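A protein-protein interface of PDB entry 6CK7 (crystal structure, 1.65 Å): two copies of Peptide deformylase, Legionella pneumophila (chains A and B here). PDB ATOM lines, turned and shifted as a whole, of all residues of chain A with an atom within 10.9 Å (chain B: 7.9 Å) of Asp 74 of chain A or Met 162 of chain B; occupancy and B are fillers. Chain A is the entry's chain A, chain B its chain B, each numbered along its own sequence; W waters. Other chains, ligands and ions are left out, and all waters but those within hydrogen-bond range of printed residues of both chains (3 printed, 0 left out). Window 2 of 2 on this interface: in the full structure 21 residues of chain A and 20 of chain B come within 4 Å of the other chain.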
ATOM      1  N   PHE A  44      19.245   0.268 -17.341  1.00  0.00           N
ATOM      2  CA  PHE A  44      19.498  -0.044 -18.749  1.00  0.00           C
ATOM      3  C   PHE A  44      20.464   0.967 -19.360  1.00  0.00           C
ATOM      4  O   PHE A  44      21.439   0.593 -20.021  1.00  0.00           O
ATOM      5  CB  PHE A  44      18.191  -0.079 -19.544  1.00  0.00           C
ATOM      6  CG  PHE A  44      17.474  -1.402 -19.494  1.00  0.00           C
ATOM      7  CD1 PHE A  44      18.014  -2.524 -20.062  1.00  0.00           C
ATOM      8  CD2 PHE A  44      16.241  -1.516 -18.882  1.00  0.00           C
ATOM      9  CE1 PHE A  44      17.317  -3.742 -20.014  1.00  0.00           C
ATOM     10  CE2 PHE A  44      15.563  -2.738 -18.841  1.00  0.00           C
ATOM     11  CZ  PHE A  44      16.109  -3.840 -19.392  1.00  0.00           C
ATOM     12  N   MET A  47      23.934   0.245 -18.047  1.00  0.00           N
ATOM     13  CA  MET A  47      24.460  -0.971 -18.655  1.00  0.00           C
ATOM     14  C   MET A  47      24.960  -0.718 -20.070  1.00  0.00           C
ATOM     15  O   MET A  47      26.093  -1.082 -20.415  1.00  0.00           O
ATOM     16  CB  MET A  47      23.370  -2.049 -18.660  1.00  0.00           C
ATOM     17  CG  MET A  47      23.812  -3.359 -19.256  1.00  0.00           C
ATOM     18  SD  MET A  47      22.369  -4.401 -19.651  1.00  0.00           S
ATOM     19  CE  MET A  47      21.864  -3.630 -21.161  1.00  0.00           C
ATOM     20  N   TYR A  48      24.126  -0.105 -20.916  1.00  0.00           N
ATOM     21  CA  TYR A  48      24.565   0.145 -22.289  1.00  0.00           C
ATOM     22  C   TYR A  48      25.746   1.103 -22.316  1.00  0.00           C
ATOM     23  O   TYR A  48      26.687   0.924 -23.105  1.00  0.00           O
ATOM     24  CB  TYR A  48      23.424   0.712 -23.136  1.00  0.00           C
ATOM     25  CG  TYR A  48      22.249  -0.218 -23.373  1.00  0.00           C
ATOM     26  CD1 TYR A  48      22.412  -1.450 -24.006  1.00  0.00           C
ATOM     27  CD2 TYR A  48      20.965   0.159 -22.993  1.00  0.00           C
ATOM     28  CE1 TYR A  48      21.316  -2.287 -24.241  1.00  0.00           C
ATOM     29  CE2 TYR A  48      19.881  -0.657 -23.214  1.00  0.00           C
ATOM     30  CZ  TYR A  48      20.058  -1.887 -23.828  1.00  0.00           C
ATOM     31  OH  TYR A  48      18.979  -2.704 -24.048  1.00  0.00           O
ATOM     32  N   GLY A  52      27.942  -3.247 -21.293  1.00  0.00           N
ATOM     33  CA  GLY A  52      27.583  -4.525 -20.712  1.00  0.00           C
ATOM     34  C   GLY A  52      26.340  -5.118 -21.357  1.00  0.00           C
ATOM     35  O   GLY A  52      25.648  -4.472 -22.143  1.00  0.00           O
ATOM     36  N   VAL A  53      26.098  -6.396 -21.051  1.00  0.00           N
ATOM     37  CA  VAL A  53      24.864  -7.056 -21.463  1.00  0.00           C
ATOM     38  C   VAL A  53      23.961  -7.371 -20.284  1.00  0.00           C
ATOM     39  O   VAL A  53      22.872  -7.940 -20.478  1.00  0.00           O
ATOM     40  CB  VAL A  53      25.146  -8.324 -22.283  1.00  0.00           C
ATOM     41  CG1 VAL A  53      25.943  -7.971 -23.515  1.00  0.00           C
ATOM     42  CG2 VAL A  53      25.885  -9.376 -21.439  1.00  0.00           C
ATOM     43  N   VAL A  68      18.835  -5.979 -14.972  1.00  0.00           N
ATOM     44  CA  VAL A  68      18.427  -5.727 -16.347  1.00  0.00           C
ATOM     45  C   VAL A  68      19.413  -6.466 -17.244  1.00  0.00           C
ATOM     46  O   VAL A  68      20.597  -6.596 -16.923  1.00  0.00           O
ATOM     47  CB  VAL A  68      18.380  -4.222 -16.688  1.00  0.00           C
ATOM     48  CG1 VAL A  68      17.366  -3.493 -15.783  1.00  0.00           C
ATOM     49  CG2 VAL A  68      19.768  -3.603 -16.572  1.00  0.00           C
ATOM     50  N   ILE A  69      18.909  -6.974 -18.362  1.00  0.00           N
ATOM     51  CA  ILE A  69      19.680  -7.830 -19.260  1.00  0.00           C
ATOM     52  C   ILE A  69      19.301  -7.492 -20.699  1.00  0.00           C
ATOM     53  O   ILE A  69      18.117  -7.367 -21.021  1.00  0.00           O
ATOM     54  CB  ILE A  69      19.394  -9.323 -18.975  1.00  0.00           C
ATOM     55  CG1 ILE A  69      19.930  -9.727 -17.608  1.00  0.00           C
ATOM     56  CG2 ILE A  69      20.006 -10.241 -20.058  1.00  0.00           C
ATOM     57  CD1 ILE A  69      19.523 -11.165 -17.237  1.00  0.00           C
ATOM     58  N   ASP A  70      20.306  -7.402 -21.584  1.00  0.00           N
ATOM     59  CA  ASP A  70      20.043  -7.370 -23.024  1.00  0.00           C
ATOM     60  C   ASP A  70      21.240  -8.007 -23.717  1.00  0.00           C
ATOM     61  O   ASP A  70      22.250  -7.337 -23.942  1.00  0.00           O
ATOM     62  CB  ASP A  70      19.835  -5.954 -23.543  1.00  0.00           C
ATOM     63  CG  ASP A  70      19.350  -5.892 -24.968  1.00  0.00           C
ATOM     64  OD1 ASP A  70      19.253  -6.928 -25.643  1.00  0.00           O
ATOM     65  OD2 ASP A  70      19.074  -4.765 -25.444  1.00  0.00           O
ATOM     66  N   ILE A  71      21.099  -9.273 -24.090  1.00  0.00           N
ATOM     67  CA  ILE A  71      22.170 -10.014 -24.750  1.00  0.00           C
ATOM     68  C   ILE A  71      22.262  -9.631 -26.218  1.00  0.00           C
ATOM     69  O   ILE A  71      23.346  -9.567 -26.803  1.00  0.00           O
ATOM     70  CB  ILE A  71      21.923 -11.526 -24.587  1.00  0.00           C
ATOM     71  CG1 ILE A  71      21.730 -11.896 -23.112  1.00  0.00           C
ATOM     72  CG2 ILE A  71      23.055 -12.330 -25.219  1.00  0.00           C
ATOM     73  CD1 ILE A  71      22.907 -11.562 -22.244  1.00  0.00           C
ATOM     74  N   VAL A  72      21.110  -9.406 -26.839  1.00  0.00           N
ATOM     75  CA  VAL A  72      21.071  -9.079 -28.257  1.00  0.00           C
ATOM     76  C   VAL A  72      21.459  -7.622 -28.478  1.00  0.00           C
ATOM     77  O   VAL A  72      22.198  -7.299 -29.413  1.00  0.00           O
ATOM     78  CB  VAL A  72      19.674  -9.395 -28.810  1.00  0.00           C
ATOM     79  CG1 VAL A  72      19.540  -8.900 -30.223  1.00  0.00           C
ATOM     80  CG2 VAL A  72      19.409 -10.894 -28.758  1.00  0.00           C
ATOM     81  N   GLY A  73      20.989  -6.726 -27.622  1.00  0.00           N
ATOM     82  CA  GLY A  73      21.364  -5.332 -27.702  1.00  0.00           C
ATOM     83  C   GLY A  73      20.305  -4.386 -28.228  1.00  0.00           C
ATOM     84  O   GLY A  73      20.632  -3.225 -28.498  1.00  0.00           O
ATOM     85  N   ASP A  74      19.053  -4.826 -28.374  1.00  0.00           N
ATOM     86  CA  ASP A  74      17.962  -3.953 -28.793  1.00  0.00           C
ATOM     87  C   ASP A  74      16.780  -4.074 -27.830  1.00  0.00           C
ATOM     88  O   ASP A  74      16.749  -4.929 -26.944  1.00  0.00           O
ATOM     89  CB  ASP A  74      17.529  -4.248 -30.233  1.00  0.00           C
ATOM     90  CG  ASP A  74      17.249  -5.719 -30.475  1.00  0.00           C
ATOM     91  OD1 ASP A  74      16.907  -6.435 -29.512  1.00  0.00           O
ATOM     92  OD2 ASP A  74      17.365  -6.158 -31.640  1.00  0.00           O
ATOM     93  N   LYS A  75      15.779  -3.212 -28.039  1.00  0.00           N
ATOM     94  CA  LYS A  75      14.726  -3.017 -27.043  1.00  0.00           C
ATOM     95  C   LYS A  75      13.769  -4.200 -26.957  1.00  0.00           C
ATOM     96  O   LYS A  75      13.220  -4.468 -25.882  1.00  0.00           O
ATOM     97  CB  LYS A  75      13.946  -1.737 -27.354  1.00  0.00           C
ATOM     98  N   LYS A  76      13.545  -4.911 -28.065  1.00  0.00           N
ATOM     99  CA  LYS A  76      12.560  -5.989 -28.069  1.00  0.00           C
ATOM    100  C   LYS A  76      13.021  -7.196 -27.266  1.00  0.00           C
ATOM    101  O   LYS A  76      12.193  -8.034 -26.896  1.00  0.00           O
ATOM    102  CB  LYS A  76      12.245  -6.411 -29.505  1.00  0.00           C
ATOM    103  CG  LYS A  76      11.009  -7.292 -29.648  1.00  0.00           C
ATOM    104  CD  LYS A  76      10.782  -7.691 -31.103  1.00  0.00           C
ATOM    105  CE  LYS A  76      10.982  -9.181 -31.311  1.00  0.00           C
ATOM    106  NZ  LYS A  76      12.425  -9.533 -31.305  1.00  0.00           N
ATOM    107  N   GLU A  77      14.320  -7.308 -26.994  1.00  0.00           N
ATOM    108  CA  GLU A  77      14.872  -8.431 -26.251  1.00  0.00           C
ATOM    109  C   GLU A  77      15.292  -8.041 -24.840  1.00  0.00           C
ATOM    110  O   GLU A  77      16.059  -8.770 -24.205  1.00  0.00           O
ATOM    111  CB  GLU A  77      16.058  -9.033 -27.008  1.00  0.00           C
ATOM    112  CG  GLU A  77      15.697  -9.646 -28.366  1.00  0.00           C
ATOM    113  CD  GLU A  77      15.403 -11.134 -28.278  1.00  0.00           C
ATOM    114  OE1 GLU A  77      15.708 -11.863 -29.247  1.00  0.00           O
ATOM    115  OE2 GLU A  77      14.869 -11.580 -27.240  1.00  0.00           O
ATOM    116  N   GLN A  78      14.829  -6.896 -24.335  1.00  0.00           N
ATOM    117  CA  GLN A  78      15.199  -6.512 -22.980  1.00  0.00           C
ATOM    118  C   GLN A  78      14.531  -7.432 -21.973  1.00  0.00           C
ATOM    119  O   GLN A  78      13.342  -7.746 -22.083  1.00  0.00           O
ATOM    120  CB  GLN A  78      14.796  -5.074 -22.677  1.00  0.00           C
ATOM    121  CG  GLN A  78      15.605  -4.035 -23.402  1.00  0.00           C
ATOM    122  CD  GLN A  78      15.237  -2.632 -22.967  1.00  0.00           C
ATOM    123  OE1 GLN A  78      14.129  -2.388 -22.463  1.00  0.00           O
ATOM    124  NE2 GLN A  78      16.157  -1.694 -23.171  1.00  0.00           N
ATOM    125  N   ILE A  79      15.301  -7.855 -20.988  1.00  0.00           N
ATOM    126  CA  ILE A  79      14.812  -8.695 -19.905  1.00  0.00           C
ATOM    127  C   ILE A  79      15.036  -7.956 -18.600  1.00  0.00           C
ATOM    128  O   ILE A  79      16.110  -7.388 -18.381  1.00  0.00           O
ATOM    129  CB  ILE A  79      15.524 -10.065 -19.878  1.00  0.00           C
ATOM    130  CG1 ILE A  79      15.242 -10.835 -21.165  1.00  0.00           C
ATOM    131  CG2 ILE A  79      15.105 -10.872 -18.656  1.00  0.00           C
ATOM    132  CD1 ILE A  79      16.266 -11.942 -21.438  1.00  0.00           C
ATOM    133  N   VAL A  80      14.030  -7.966 -17.731  1.00  0.00           N
ATOM    134  CA  VAL A  80      14.186  -7.520 -16.352  1.00  0.00           C
ATOM    135  C   VAL A  80      13.826  -8.689 -15.450  1.00  0.00           C
ATOM    136  O   VAL A  80      12.755  -9.281 -15.604  1.00  0.00           O
ATOM    137  CB  VAL A  80      13.304  -6.294 -16.038  1.00  0.00           C
ATOM    138  CG1 VAL A  80      13.478  -5.879 -14.579  1.00  0.00           C
ATOM    139  CG2 VAL A  80      13.645  -5.148 -16.981  1.00  0.00           C
ATOM    140  N   ARG A 122       9.297  -6.370 -15.030  1.00  0.00           N
ATOM    141  CA  ARG A 122       9.486  -5.011 -14.532  1.00  0.00           C
ATOM    142  C   ARG A 122       8.202  -4.406 -13.977  1.00  0.00           C
ATOM    143  O   ARG A 122       8.270  -3.389 -13.277  1.00  0.00           O
ATOM    144  CB  ARG A 122      10.059  -4.112 -15.634  1.00  0.00           C
ATOM    145  CG  ARG A 122       9.102  -3.801 -16.779  1.00  0.00           C
ATOM    146  CD  ARG A 122       9.804  -2.931 -17.824  1.00  0.00           C
ATOM    147  NE  ARG A 122      10.118  -1.625 -17.253  1.00  0.00           N
ATOM    148  CZ  ARG A 122      11.056  -0.792 -17.694  1.00  0.00           C
ATOM    149  NH1 ARG A 122      11.814  -1.105 -18.750  1.00  0.00           N
ATOM    150  NH2 ARG A 122      11.235   0.373 -17.082  1.00  0.00           N
ATOM    151  N   GLY B 104      30.099  -1.550 -27.364  1.00  0.00           N
ATOM    152  CA  GLY B 104      28.792  -2.109 -27.143  1.00  0.00           C
ATOM    153  C   GLY B 104      28.450  -3.279 -28.029  1.00  0.00           C
ATOM    154  O   GLY B 104      27.534  -4.035 -27.702  1.00  0.00           O
ATOM    155  N   ALA B 105      29.156  -3.453 -29.140  1.00  0.00           N
ATOM    156  CA  ALA B 105      28.838  -4.510 -30.088  1.00  0.00           C
ATOM    157  C   ALA B 105      29.585  -5.780 -29.703  1.00  0.00           C
ATOM    158  O   ALA B 105      30.812  -5.771 -29.564  1.00  0.00           O
ATOM    159  CB  ALA B 105      29.203  -4.084 -31.511  1.00  0.00           C
ATOM    160  N   ASP B 107      29.676  -9.920 -30.974  1.00  0.00           N
ATOM    161  CA  ASP B 107      29.146 -10.870 -31.939  1.00  0.00           C
ATOM    162  C   ASP B 107      30.090 -12.050 -32.043  1.00  0.00           C
ATOM    163  O   ASP B 107      31.261 -11.971 -31.670  1.00  0.00           O
ATOM    164  CB  ASP B 107      28.999 -10.267 -33.348  1.00  0.00           C
ATOM    165  CG  ASP B 107      27.831  -9.326 -33.468  1.00  0.00           C
ATOM    166  OD1 ASP B 107      26.701  -9.803 -33.697  1.00  0.00           O
ATOM    167  OD2 ASP B 107      28.058  -8.103 -33.346  1.00  0.00           O
ATOM    168  N   VAL B 152      33.096  -6.218 -37.378  1.00  0.00           N
ATOM    169  CA  VAL B 152      31.732  -6.166 -37.872  1.00  0.00           C
ATOM    170  C   VAL B 152      31.662  -6.383 -39.371  1.00  0.00           C
ATOM    171  O   VAL B 152      30.618  -6.810 -39.876  1.00  0.00           O
ATOM    172  CB  VAL B 152      31.086  -4.828 -37.487  1.00  0.00           C
ATOM    173  CG1 VAL B 152      30.880  -4.768 -35.967  1.00  0.00           C
ATOM    174  CG2 VAL B 152      31.941  -3.658 -37.968  1.00  0.00           C
ATOM    175  N   LEU B 155      30.340  -9.725 -40.544  1.00  0.00           N
ATOM    176  CA  LEU B 155      29.007 -10.147 -40.134  1.00  0.00           C
ATOM    177  C   LEU B 155      27.990  -9.978 -41.262  1.00  0.00           C
ATOM    178  O   LEU B 155      28.214  -9.268 -42.245  1.00  0.00           O
ATOM    179  CB  LEU B 155      28.536  -9.347 -38.914  1.00  0.00           C
ATOM    180  CG  LEU B 155      29.453  -9.341 -37.687  1.00  0.00           C
ATOM    181  CD1 LEU B 155      28.956  -8.335 -36.659  1.00  0.00           C
ATOM    182  CD2 LEU B 155      29.552 -10.734 -37.080  1.00  0.00           C
ATOM    183  N   SER B 156      26.843 -10.639 -41.091  1.00  0.00           N
ATOM    184  CA  SER B 156      25.743 -10.493 -42.037  1.00  0.00           C
ATOM    185  C   SER B 156      25.234  -9.052 -42.040  1.00  0.00           C
ATOM    186  O   SER B 156      25.436  -8.315 -41.074  1.00  0.00           O
ATOM    187  CB  SER B 156      24.603 -11.440 -41.668  1.00  0.00           C
ATOM    188  OG  SER B 156      24.062 -11.084 -40.403  1.00  0.00           O
ATOM    189  N   PRO B 157      24.580  -8.623 -43.128  1.00  0.00           N
ATOM    190  CA  PRO B 157      24.003  -7.266 -43.142  1.00  0.00           C
ATOM    191  C   PRO B 157      23.077  -6.987 -41.968  1.00  0.00           C
ATOM    192  O   PRO B 157      23.126  -5.892 -41.388  1.00  0.00           O
ATOM    193  CB  PRO B 157      23.263  -7.224 -44.489  1.00  0.00           C
ATOM    194  CG  PRO B 157      24.072  -8.138 -45.359  1.00  0.00           C
ATOM    195  CD  PRO B 157      24.504  -9.269 -44.450  1.00  0.00           C
ATOM    196  N   LEU B 158      22.248  -7.961 -41.585  1.00  0.00           N
ATOM    197  CA  LEU B 158      21.396  -7.793 -40.409  1.00  0.00           C
ATOM    198  C   LEU B 158      22.228  -7.510 -39.162  1.00  0.00           C
ATOM    199  O   LEU B 158      21.941  -6.570 -38.411  1.00  0.00           O
ATOM    200  CB  LEU B 158      20.530  -9.038 -40.213  1.00  0.00           C
ATOM    201  CG  LEU B 158      19.749  -9.151 -38.902  1.00  0.00           C
ATOM    202  CD1 LEU B 158      18.723  -8.037 -38.785  1.00  0.00           C
ATOM    203  CD2 LEU B 158      19.071 -10.509 -38.793  1.00  0.00           C
ATOM    204  N   LYS B 159      23.278  -8.307 -38.930  1.00  0.00           N
ATOM    205  CA  LYS B 159      24.084  -8.111 -37.729  1.00  0.00           C
ATOM    206  C   LYS B 159      24.873  -6.811 -37.790  1.00  0.00           C
ATOM    207  O   LYS B 159      25.110  -6.184 -36.751  1.00  0.00           O
ATOM    208  CB  LYS B 159      25.031  -9.293 -37.519  1.00  0.00           C
ATOM    209  CG  LYS B 159      24.321 -10.577 -37.093  1.00  0.00           C
ATOM    210  CD  LYS B 159      25.315 -11.687 -36.809  1.00  0.00           C
ATOM    211  CE  LYS B 159      24.624 -12.890 -36.187  1.00  0.00           C
ATOM    212  NZ  LYS B 159      23.845 -12.508 -34.981  1.00  0.00           N
ATOM    213  N   ARG B 160      25.293  -6.395 -38.991  1.00  0.00           N
ATOM    214  CA  ARG B 160      25.991  -5.119 -39.104  1.00  0.00           C
ATOM    215  C   ARG B 160      25.063  -3.967 -38.769  1.00  0.00           C
ATOM    216  O   ARG B 160      25.473  -3.007 -38.108  1.00  0.00           O
ATOM    217  CB  ARG B 160      26.573  -4.945 -40.511  1.00  0.00           C
ATOM    218  CG  ARG B 160      27.596  -5.992 -40.851  1.00  0.00           C
ATOM    219  CD  ARG B 160      28.544  -5.543 -41.957  1.00  0.00           C
ATOM    220  NE  ARG B 160      27.864  -5.084 -43.168  1.00  0.00           N
ATOM    221  CZ  ARG B 160      27.480  -5.871 -44.171  1.00  0.00           C
ATOM    222  NH1 ARG B 160      27.671  -7.189 -44.127  1.00  0.00           N
ATOM    223  NH2 ARG B 160      26.909  -5.341 -45.233  1.00  0.00           N
ATOM    224  N   MET B 161      23.809  -4.049 -39.218  1.00  0.00           N
ATOM    225  CA  MET B 161      22.840  -3.008 -38.894  1.00  0.00           C
ATOM    226  C   MET B 161      22.577  -2.962 -37.397  1.00  0.00           C
ATOM    227  O   MET B 161      22.526  -1.880 -36.800  1.00  0.00           O
ATOM    228  CB  MET B 161      21.543  -3.241 -39.670  1.00  0.00           C
ATOM    229  N   MET B 162      22.426  -4.130 -36.767  1.00  0.00           N
ATOM    230  CA  MET B 162      22.175  -4.156 -35.331  1.00  0.00           C
ATOM    231  C   MET B 162      23.359  -3.602 -34.549  1.00  0.00           C
ATOM    232  O   MET B 162      23.170  -2.958 -33.507  1.00  0.00           O
ATOM    233  CB  MET B 162      21.854  -5.577 -34.875  1.00  0.00           C
ATOM    234  CG  MET B 162      20.682  -6.201 -35.610  1.00  0.00           C
ATOM    235  SD  MET B 162      20.350  -7.882 -35.064  1.00  0.00           S
ATOM    236  CE  MET B 162      19.843  -7.540 -33.383  1.00  0.00           C
ATOM    237  N   ALA B 163      24.585  -3.843 -35.028  1.00  0.00           N
ATOM    238  CA  ALA B 163      25.754  -3.295 -34.346  1.00  0.00           C
ATOM    239  C   ALA B 163      25.829  -1.785 -34.518  1.00  0.00           C
ATOM    240  O   ALA B 163      26.216  -1.069 -33.589  1.00  0.00           O
ATOM    241  CB  ALA B 163      27.036  -3.964 -34.847  1.00  0.00           C
ATOM    242  N   ARG B 164      25.458  -1.282 -35.700  1.00  0.00           N
ATOM    243  CA  ARG B 164      25.415   0.161 -35.936  1.00  0.00           C
ATOM    244  C   ARG B 164      24.436   0.846 -34.991  1.00  0.00           C
ATOM    245  O   ARG B 164      24.744   1.892 -34.408  1.00  0.00           O
ATOM    246  CB  ARG B 164      25.021   0.444 -37.387  1.00  0.00           C
ATOM    247  CG  ARG B 164      26.160   0.869 -38.299  1.00  0.00           C
ATOM    248  CD  ARG B 164      25.636   1.600 -39.551  1.00  0.00           C
ATOM    249  NE  ARG B 164      24.553   0.886 -40.229  1.00  0.00           N
ATOM    250  CZ  ARG B 164      24.735  -0.113 -41.092  1.00  0.00           C
ATOM    251  NH1 ARG B 164      25.960  -0.526 -41.387  1.00  0.00           N
ATOM    252  NH2 ARG B 164      23.691  -0.704 -41.659  1.00  0.00           N
ATOM    253  N   ARG B 165      23.237   0.281 -34.842  1.00  0.00           N
ATOM    254  CA  ARG B 165      22.236   0.937 -34.008  1.00  0.00           C
ATOM    255  C   ARG B 165      22.630   0.870 -32.540  1.00  0.00           C
ATOM    256  O   ARG B 165      22.413   1.830 -31.793  1.00  0.00           O
ATOM    257  CB  ARG B 165      20.857   0.321 -34.249  1.00  0.00           C
ATOM    258  CG  ARG B 165      20.444   0.370 -35.715  1.00  0.00           C
ATOM    259  CD  ARG B 165      18.964   0.115 -35.925  1.00  0.00           C
ATOM    260  NE  ARG B 165      18.155   1.311 -35.711  1.00  0.00           N
ATOM    261  CZ  ARG B 165      17.237   1.430 -34.755  1.00  0.00           C
ATOM    262  NH1 ARG B 165      17.012   0.426 -33.918  1.00  0.00           N
ATOM    263  NH2 ARG B 165      16.546   2.555 -34.635  1.00  0.00           N
ATOM    264  N   LYS B 166      23.246  -0.236 -32.124  1.00  0.00           N
ATOM    265  CA  LYS B 166      23.748  -0.332 -30.754  1.00  0.00           C
ATOM    266  C   LYS B 166      24.846   0.693 -30.504  1.00  0.00           C
ATOM    267  O   LYS B 166      24.914   1.304 -29.430  1.00  0.00           O
ATOM    268  CB  LYS B 166      24.267  -1.739 -30.495  1.00  0.00           C
ATOM    269  CG  LYS B 166      24.673  -1.954 -29.068  1.00  0.00           C
ATOM    270  CD  LYS B 166      24.655  -3.411 -28.682  1.00  0.00           C
ATOM    271  CE  LYS B 166      24.548  -3.503 -27.179  1.00  0.00           C
ATOM    272  NZ  LYS B 166      25.138  -4.763 -26.633  1.00  0.00           N
ATOM    273  N   LEU B 167      25.721   0.886 -31.487  1.00  0.00           N
ATOM    274  CA  LEU B 167      26.769   1.891 -31.367  1.00  0.00           C
ATOM    275  C   LEU B 167      26.187   3.299 -31.349  1.00  0.00           C
ATOM    276  O   LEU B 167      26.682   4.170 -30.623  1.00  0.00           O
ATOM    277  CB  LEU B 167      27.769   1.734 -32.517  1.00  0.00           C
ATOM    278  CG  LEU B 167      28.865   2.791 -32.647  1.00  0.00           C
ATOM    279  CD1 LEU B 167      29.705   2.878 -31.375  1.00  0.00           C
ATOM    280  CD2 LEU B 167      29.724   2.468 -33.855  1.00  0.00           C
ATOM    281  N   ASP B 168      25.153   3.553 -32.158  1.00  0.00           N
ATOM    282  CA  ASP B 168      24.523   4.870 -32.134  1.00  0.00           C
ATOM    283  C   ASP B 168      23.873   5.143 -30.782  1.00  0.00           C
ATOM    284  O   ASP B 168      23.917   6.274 -30.288  1.00  0.00           O
ATOM    285  CB  ASP B 168      23.486   4.994 -33.247  1.00  0.00           C
ATOM    286  CG  ASP B 168      24.119   5.077 -34.615  1.00  0.00           C
ATOM    287  OD1 ASP B 168      25.354   5.254 -34.688  1.00  0.00           O
ATOM    288  OD2 ASP B 168      23.379   4.963 -35.612  1.00  0.00           O
ATOM    289  N   LYS B 169      23.242   4.129 -30.186  1.00  0.00           N
ATOM    290  CA  LYS B 169      22.639   4.315 -28.866  1.00  0.00           C
ATOM    291  C   LYS B 169      23.708   4.593 -27.816  1.00  0.00           C
ATOM    292  O   LYS B 169      23.512   5.428 -26.923  1.00  0.00           O
ATOM    293  CB  LYS B 169      21.809   3.090 -28.486  1.00  0.00           C
ATOM    294  CG  LYS B 169      21.505   2.979 -26.989  1.00  0.00           C
ATOM    295  CD  LYS B 169      20.083   2.499 -26.729  1.00  0.00           C
ATOM    296  CE  LYS B 169      19.609   2.855 -25.318  1.00  0.00           C
ATOM    297  NZ  LYS B 169      18.177   2.524 -25.167  1.00  0.00           N
HETATM  298  O   HOH W   1      25.164  -7.269 -27.688  1.00  0.00           O
HETATM  299  O   HOH W   2      26.648  -3.276 -24.522  1.00  0.00           O
HETATM  300  O   HOH W   3      23.673  -4.887 -24.275  1.00  0.00           O
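Water W1 lies within hydrogen-bond range of the side-chain amino group of Lys 166 of chain B (2.7 Å), the backbone carbonyl oxygen of Ile 71 of chain A (3.1 Å) and the backbone carbonyl oxygen of Val 72 of chain A (3.4 Å). Water W3 lies within hydrogen-bond range of the side-chain amino group (NZ) of Lys 166 of chain B, the backbone carbonyl oxygen (O) of Asp 70 of chain A and the backbone carbonyl oxygen (O) of Gly 52 of chain A. Water W2 lies within hydrogen-bond range of O of Gly 52 of chain A (2.8 Å), NZ of Lys 166 of chain B (3.0 Å) and O of Gly 104 of chain B (3.4 Å).
Of the printed residues of chain B, Tyr 48 of chain A touches Lys 169 (3.8 Å). Asp 70 of chain A touches none of the printed residues of chain B. Of the printed residues of chain B, Asp 74 of chain A touches Met 162. Ile 79 of chain A touches none of the printed residues of chain B. No residue of chain A comes within 4 Å of Leu 158 of chain B. No residue of chain A comes within 4 Å of Lys 159 of chain B. No residue of chain A comes within 4 Å of Met 161 of chain B. Printed residues of chain A within 4 Å of Met 162 of chain B: Val 72 and Asp 74. No residue of chain A comes within 4 Å of Ala 163 of chain B. Of the printed residues of chain A, Lys 169 of chain B touches Tyr 48. The nearest printed residue of chain B that does not touch Asp 74 of chain A is Lys 166 of chain B (5.8 Å). The nearest printed residue of chain A that does not touch Lys 169 of chain B is Gln 78 of chain A (5.1 Å).
Hydrophobic or aromatic side chains of chain A within 4 Å of the printed part of chain B: Tyr 48 and Val 72. Among the printed residues, 4 pairs touch across the chains. Among the printed residues, no Asp or Glu carboxylate lies within 4 Å of a Lys or Arg side-chain nitrogen of the other chain.
Lys 169 of chain B touches Tyr 48 of chain A. Met 162 of chain B touches Val 72 of chain A (CE to CG1, 3.5 Å). Gly 73 of chain A touches Lys 166 of chain B (CA to CE, 3.7 Å). Met 162 of chain B touches Asp 74 of chain A (CE to OD2, 3.3 Å).
The side-chain carboxylate of Asp 70 of chain A is in hydrogen-bond range of the side-chain hydroxyl of Tyr 48 of chain A (2.5 Å). The backbone NH of Gly 73 of chain A sits at hydrogen-bond distance from the side-chain carboxylate of Asp 70 of chain A (2.6 Å). The backbone NH (N) of Val 72 of chain A sits at hydrogen-bond distance from the side-chain carboxylate (OD1) of Asp 70 of chain A (3.3 Å). O of Gly 104 of chain B lies within hydrogen-bond range of NZ of Lys 166 of chain B, 2.7 Å away. The side-chain hydroxyl (OH) of Tyr 48 of chain A sits at hydrogen-bond distance from the side-chain amide nitrogen (NE2) of Gln 78 of chain A (3.1 Å). OD2 of Asp 70 of chain A sits at hydrogen-bond distance from N of Asp 74 of chain A (2.9 Å).
No position is printed for both chains.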
